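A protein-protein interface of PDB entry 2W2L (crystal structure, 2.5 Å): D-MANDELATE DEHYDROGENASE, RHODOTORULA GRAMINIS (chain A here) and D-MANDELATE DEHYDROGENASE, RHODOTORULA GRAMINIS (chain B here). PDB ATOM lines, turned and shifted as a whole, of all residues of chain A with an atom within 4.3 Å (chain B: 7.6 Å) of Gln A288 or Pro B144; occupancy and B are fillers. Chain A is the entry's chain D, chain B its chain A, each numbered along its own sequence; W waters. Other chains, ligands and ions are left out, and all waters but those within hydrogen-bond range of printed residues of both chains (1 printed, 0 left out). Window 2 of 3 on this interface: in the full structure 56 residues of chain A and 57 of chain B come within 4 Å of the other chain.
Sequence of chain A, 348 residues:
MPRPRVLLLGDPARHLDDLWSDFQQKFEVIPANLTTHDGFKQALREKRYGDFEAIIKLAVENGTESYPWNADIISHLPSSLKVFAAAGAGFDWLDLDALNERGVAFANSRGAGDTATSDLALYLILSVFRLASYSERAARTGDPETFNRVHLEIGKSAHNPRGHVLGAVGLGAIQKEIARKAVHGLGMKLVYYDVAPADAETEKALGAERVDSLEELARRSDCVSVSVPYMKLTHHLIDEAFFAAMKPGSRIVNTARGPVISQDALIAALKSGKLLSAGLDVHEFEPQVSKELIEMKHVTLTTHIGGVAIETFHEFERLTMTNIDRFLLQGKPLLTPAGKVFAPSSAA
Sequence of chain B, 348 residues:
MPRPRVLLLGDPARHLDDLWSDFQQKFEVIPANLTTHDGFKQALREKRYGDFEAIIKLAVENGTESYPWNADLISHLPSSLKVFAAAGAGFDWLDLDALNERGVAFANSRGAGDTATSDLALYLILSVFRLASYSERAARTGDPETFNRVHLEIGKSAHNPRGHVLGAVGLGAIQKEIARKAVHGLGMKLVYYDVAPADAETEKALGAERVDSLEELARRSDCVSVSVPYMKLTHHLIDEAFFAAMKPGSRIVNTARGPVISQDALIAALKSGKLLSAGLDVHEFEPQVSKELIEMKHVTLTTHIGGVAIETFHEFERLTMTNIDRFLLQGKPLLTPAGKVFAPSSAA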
ATOM      1  N   PHE A 285      -5.026 -27.354   2.482  1.00  0.00           N
ATOM      2  CA  PHE A 285      -5.462 -25.954   2.663  1.00  0.00           C
ATOM      3  C   PHE A 285      -5.418 -25.505   4.088  1.00  0.00           C
ATOM      4  O   PHE A 285      -6.308 -24.775   4.526  1.00  0.00           O
ATOM      5  CB  PHE A 285      -6.849 -25.690   2.099  1.00  0.00           C
ATOM      6  CG  PHE A 285      -6.997 -26.098   0.673  1.00  0.00           C
ATOM      7  CD1 PHE A 285      -7.802 -27.194   0.333  1.00  0.00           C
ATOM      8  CD2 PHE A 285      -6.322 -25.409  -0.332  1.00  0.00           C
ATOM      9  CE1 PHE A 285      -7.927 -27.607  -0.989  1.00  0.00           C
ATOM     10  CE2 PHE A 285      -6.442 -25.798  -1.681  1.00  0.00           C
ATOM     11  CZ  PHE A 285      -7.233 -26.896  -2.013  1.00  0.00           C
ATOM     12  N   GLU A 286      -4.365 -25.932   4.794  1.00  0.00           N
ATOM     13  CA  GLU A 286      -4.113 -25.589   6.201  1.00  0.00           C
ATOM     14  C   GLU A 286      -4.143 -24.060   6.394  1.00  0.00           C
ATOM     15  O   GLU A 286      -3.544 -23.354   5.597  1.00  0.00           O
ATOM     16  CB  GLU A 286      -2.746 -26.149   6.590  1.00  0.00           C
ATOM     17  CG  GLU A 286      -2.774 -26.958   7.847  1.00  0.00           C
ATOM     18  CD  GLU A 286      -1.411 -27.396   8.299  1.00  0.00           C
ATOM     19  OE1 GLU A 286      -0.807 -26.643   9.085  1.00  0.00           O
ATOM     20  OE2 GLU A 286      -0.934 -28.480   7.859  1.00  0.00           O
ATOM     21  N   PRO A 287      -4.831 -23.526   7.436  1.00  0.00           N
ATOM     22  CA  PRO A 287      -5.598 -24.084   8.556  1.00  0.00           C
ATOM     23  C   PRO A 287      -7.013 -24.574   8.290  1.00  0.00           C
ATOM     24  O   PRO A 287      -7.713 -24.913   9.266  1.00  0.00           O
ATOM     25  CB  PRO A 287      -5.653 -22.928   9.570  1.00  0.00           C
ATOM     26  CG  PRO A 287      -5.461 -21.694   8.792  1.00  0.00           C
ATOM     27  CD  PRO A 287      -4.776 -22.048   7.495  1.00  0.00           C
ATOM     28  N   GLN A 288      -7.440 -24.622   7.023  1.00  0.00           N
ATOM     29  CA  GLN A 288      -8.773 -25.145   6.670  1.00  0.00           C
ATOM     30  C   GLN A 288      -8.798 -26.683   6.454  1.00  0.00           C
ATOM     31  O   GLN A 288      -8.299 -27.175   5.426  1.00  0.00           O
ATOM     32  CB  GLN A 288      -9.270 -24.478   5.388  1.00  0.00           C
ATOM     33  CG  GLN A 288     -10.688 -24.919   5.011  1.00  0.00           C
ATOM     34  CD  GLN A 288     -11.687 -24.562   6.140  1.00  0.00           C
ATOM     35  OE1 GLN A 288     -11.920 -23.376   6.433  1.00  0.00           O
ATOM     36  NE2 GLN A 288     -12.229 -25.580   6.793  1.00  0.00           N
ATOM     37  N   VAL A 289      -9.361 -27.455   7.392  1.00  0.00           N
ATOM     38  CA  VAL A 289      -9.415 -28.923   7.178  1.00  0.00           C
ATOM     39  C   VAL A 289     -10.506 -29.225   6.140  1.00  0.00           C
ATOM     40  O   VAL A 289     -11.472 -28.448   5.985  1.00  0.00           O
ATOM     41  CB  VAL A 289      -9.604 -29.729   8.500  1.00  0.00           C
ATOM     42  CG1 VAL A 289     -10.147 -31.141   8.241  1.00  0.00           C
ATOM     43  CG2 VAL A 289      -8.307 -29.816   9.277  1.00  0.00           C
ATOM     44  N   SER A 290     -10.353 -30.315   5.390  1.00  0.00           N
ATOM     45  CA  SER A 290     -11.399 -30.638   4.418  1.00  0.00           C
ATOM     46  C   SER A 290     -12.733 -30.989   5.106  1.00  0.00           C
ATOM     47  O   SER A 290     -12.826 -31.962   5.876  1.00  0.00           O
ATOM     48  CB  SER A 290     -10.977 -31.769   3.496  1.00  0.00           C
ATOM     49  OG  SER A 290     -12.122 -32.294   2.843  1.00  0.00           O
ATOM     50  N   ALA B 138     -10.572 -30.751  17.761  1.00  0.00           N
ATOM     51  CA  ALA B 138     -10.215 -29.448  17.196  1.00  0.00           C
ATOM     52  C   ALA B 138     -10.200 -29.458  15.665  1.00  0.00           C
ATOM     53  O   ALA B 138     -10.754 -28.549  15.031  1.00  0.00           O
ATOM     54  CB  ALA B 138      -8.884 -28.993  17.747  1.00  0.00           C
ATOM     55  N   ALA B 139      -9.599 -30.488  15.056  1.00  0.00           N
ATOM     56  CA  ALA B 139      -9.620 -30.557  13.592  1.00  0.00           C
ATOM     57  C   ALA B 139     -11.042 -30.617  12.978  1.00  0.00           C
ATOM     58  O   ALA B 139     -11.315 -30.004  11.922  1.00  0.00           O
ATOM     59  CB  ALA B 139      -8.809 -31.687  13.129  1.00  0.00           C
ATOM     60  N   THR B 141     -13.946 -29.505  13.895  1.00  0.00           N
ATOM     61  CA  THR B 141     -14.741 -28.269  13.885  1.00  0.00           C
ATOM     62  C   THR B 141     -14.685 -27.708  12.499  1.00  0.00           C
ATOM     63  O   THR B 141     -15.607 -27.026  12.089  1.00  0.00           O
ATOM     64  CB  THR B 141     -14.186 -27.143  14.803  1.00  0.00           C
ATOM     65  OG1 THR B 141     -12.952 -26.658  14.261  1.00  0.00           O
ATOM     66  CG2 THR B 141     -13.978 -27.630  16.211  1.00  0.00           C
ATOM     67  N   GLY B 142     -13.588 -27.955  11.788  1.00  0.00           N
ATOM     68  CA  GLY B 142     -13.396 -27.372  10.446  1.00  0.00           C
ATOM     69  C   GLY B 142     -13.400 -25.845  10.479  1.00  0.00           C
ATOM     70  O   GLY B 142     -13.658 -25.174   9.476  1.00  0.00           O
ATOM     71  N   ASP B 143     -13.130 -25.316  11.667  1.00  0.00           N
ATOM     72  CA  ASP B 143     -12.978 -23.904  11.899  1.00  0.00           C
ATOM     73  C   ASP B 143     -11.477 -23.618  12.009  1.00  0.00           C
ATOM     74  O   ASP B 143     -10.819 -24.047  12.958  1.00  0.00           O
ATOM     75  CB  ASP B 143     -13.715 -23.535  13.187  1.00  0.00           C
ATOM     76  CG  ASP B 143     -13.688 -22.023  13.499  1.00  0.00           C
ATOM     77  OD1 ASP B 143     -13.224 -21.167  12.659  1.00  0.00           O
ATOM     78  OD2 ASP B 143     -14.161 -21.687  14.633  1.00  0.00           O
ATOM     79  N   PRO B 144     -10.932 -22.894  11.018  1.00  0.00           N
ATOM     80  CA  PRO B 144      -9.526 -22.415  10.933  1.00  0.00           C
ATOM     81  C   PRO B 144      -8.951 -21.833  12.231  1.00  0.00           C
ATOM     82  O   PRO B 144      -7.789 -22.128  12.600  1.00  0.00           O
ATOM     83  CB  PRO B 144      -9.617 -21.327   9.871  1.00  0.00           C
ATOM     84  CG  PRO B 144     -10.677 -21.867   8.930  1.00  0.00           C
ATOM     85  CD  PRO B 144     -11.716 -22.484   9.833  1.00  0.00           C
ATOM     86  N   GLU B 145      -9.757 -21.019  12.926  1.00  0.00           N
ATOM     87  CA  GLU B 145      -9.291 -20.436  14.185  1.00  0.00           C
ATOM     88  C   GLU B 145      -9.108 -21.458  15.279  1.00  0.00           C
ATOM     89  O   GLU B 145      -8.058 -21.443  15.956  1.00  0.00           O
ATOM     90  CB  GLU B 145     -10.123 -19.259  14.661  1.00  0.00           C
ATOM     91  CG  GLU B 145      -9.706 -17.940  13.992  1.00  0.00           C
ATOM     92  CD  GLU B 145      -8.175 -17.640  14.049  1.00  0.00           C
ATOM     93  OE1 GLU B 145      -7.503 -17.866  15.095  1.00  0.00           O
ATOM     94  OE2 GLU B 145      -7.648 -17.138  13.022  1.00  0.00           O
ATOM     95  N   THR B 146     -10.093 -22.357  15.432  1.00  0.00           N
ATOM     96  CA  THR B 146      -9.960 -23.505  16.356  1.00  0.00           C
ATOM     97  C   THR B 146      -8.671 -24.314  16.060  1.00  0.00           C
ATOM     98  O   THR B 146      -7.843 -24.528  16.962  1.00  0.00           O
ATOM     99  CB  THR B 146     -11.218 -24.365  16.336  1.00  0.00           C
ATOM    100  OG1 THR B 146     -12.373 -23.504  16.339  1.00  0.00           O
ATOM    101  CG2 THR B 146     -11.276 -25.325  17.564  1.00  0.00           C
ATOM    102  N   PHE B 147      -8.483 -24.695  14.796  1.00  0.00           N
ATOM    103  CA  PHE B 147      -7.258 -25.345  14.369  1.00  0.00           C
ATOM    104  C   PHE B 147      -6.022 -24.682  14.986  1.00  0.00           C
ATOM    105  O   PHE B 147      -5.278 -25.348  15.745  1.00  0.00           O
ATOM    106  CB  PHE B 147      -7.158 -25.363  12.841  1.00  0.00           C
ATOM    107  CG  PHE B 147      -6.024 -26.194  12.306  1.00  0.00           C
ATOM    108  CD1 PHE B 147      -6.278 -27.417  11.656  1.00  0.00           C
ATOM    109  CD2 PHE B 147      -4.704 -25.773  12.424  1.00  0.00           C
ATOM    110  CE1 PHE B 147      -5.215 -28.221  11.137  1.00  0.00           C
ATOM    111  CE2 PHE B 147      -3.644 -26.568  11.908  1.00  0.00           C
ATOM    112  CZ  PHE B 147      -3.907 -27.793  11.274  1.00  0.00           C
ATOM    113  N   ASN B 148      -5.791 -23.394  14.686  1.00  0.00           N
ATOM    114  CA  ASN B 148      -4.629 -22.694  15.259  1.00  0.00           C
ATOM    115  C   ASN B 148      -4.582 -22.508  16.760  1.00  0.00           C
ATOM    116  O   ASN B 148      -3.510 -22.627  17.360  1.00  0.00           O
ATOM    117  CB  ASN B 148      -4.441 -21.348  14.626  1.00  0.00           C
ATOM    118  CG  ASN B 148      -4.061 -21.450  13.202  1.00  0.00           C
ATOM    119  OD1 ASN B 148      -3.390 -22.436  12.764  1.00  0.00           O
ATOM    120  ND2 ASN B 148      -4.499 -20.444  12.422  1.00  0.00           N
ATOM    121  N   ARG B 149      -5.722 -22.179  17.377  1.00  0.00           N
ATOM    122  CA  ARG B 149      -5.713 -21.978  18.815  1.00  0.00           C
ATOM    123  C   ARG B 149      -5.356 -23.284  19.525  1.00  0.00           C
ATOM    124  O   ARG B 149      -4.588 -23.284  20.494  1.00  0.00           O
ATOM    125  CB  ARG B 149      -7.022 -21.384  19.332  1.00  0.00           C
ATOM    126  CG  ARG B 149      -6.979 -20.914  20.827  1.00  0.00           C
ATOM    127  CD  ARG B 149      -8.191 -21.431  21.620  1.00  0.00           C
ATOM    128  NE  ARG B 149      -9.299 -21.690  20.688  1.00  0.00           N
ATOM    129  CZ  ARG B 149     -10.192 -22.690  20.766  1.00  0.00           C
ATOM    130  NH1 ARG B 149     -10.163 -23.574  21.770  1.00  0.00           N
ATOM    131  NH2 ARG B 149     -11.143 -22.791  19.830  1.00  0.00           N
ATOM    132  N   VAL B 150      -5.871 -24.405  19.022  1.00  0.00           N
ATOM    133  CA  VAL B 150      -5.637 -25.680  19.679  1.00  0.00           C
ATOM    134  C   VAL B 150      -4.244 -26.185  19.362  1.00  0.00           C
ATOM    135  O   VAL B 150      -3.560 -26.719  20.247  1.00  0.00           O
ATOM    136  CB  VAL B 150      -6.733 -26.677  19.371  1.00  0.00           C
ATOM    137  CG1 VAL B 150      -6.436 -28.019  19.995  1.00  0.00           C
ATOM    138  CG2 VAL B 150      -8.084 -26.143  19.914  1.00  0.00           C
HETATM  139  O   HOH W   1     -10.371 -26.377   9.950  1.00  0.00           O
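Water W1 lies within hydrogen-bond range of the backbone NH (N) of Val A289, the backbone carbonyl oxygen (O) of Pro A287 and the backbone NH (N) of Asp B143.
Hydrophobic or aromatic side chains of chain B that line the printed part of chain A: Pro B144 and Phe B147.
Printed residues of chain A that touch a printed residue of chain B: Glu A286, Pro A287, Gln A288 and Val A289.
Hydrophobic or aromatic side chains of chain A within 4 Å of the printed part of chain B: Pro A287 and Val A289.
Among the printed residues, 8 pairs touch across the chains.
Among the printed residues, no Asp or Glu carboxylate lies within 4 Å of a Lys or Arg side-chain nitrogen of the other chain.
The side-chain amide nitrogen (NE2) of Gln A288 is in hydrogen-bond range of the backbone carbonyl oxygen (O) of Gly B142 (3.1 Å).
Of the printed residues of chain B, Glu A286 touches Phe B147.
Gln A288 touches just these residues of chain B: Gly B142 (3.1 Å) and Pro B144 (3.2 Å).
Ala B138 touches none of the printed residues of chain A.
Of chain A, only Pro A287 and Gln A288 come within 4 Å of Pro B144.
Thr B146 touches none of the printed residues of chain A.
Printed residues of chain A within 4 Å of Asn B148: Pro A287 (3.9 Å).
The nearest printed residue of chain A that does not touch Pro B144 is Val A289 (5.9 Å).
Among the printed residues, pairs that only touch across the chains: Gln A288 with Pro B144 (3.2 Å), Pro A287 with Pro B144 (3.5 Å), Pro A287 with Phe B147 (3.6 Å), Glu A286 with Phe B147 (3.7 Å), Val A289 with Ala B139 (3.8 Å), Val A289 with Phe B147 (3.9 Å) and Pro A287 with Asn B148 (3.9 Å).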
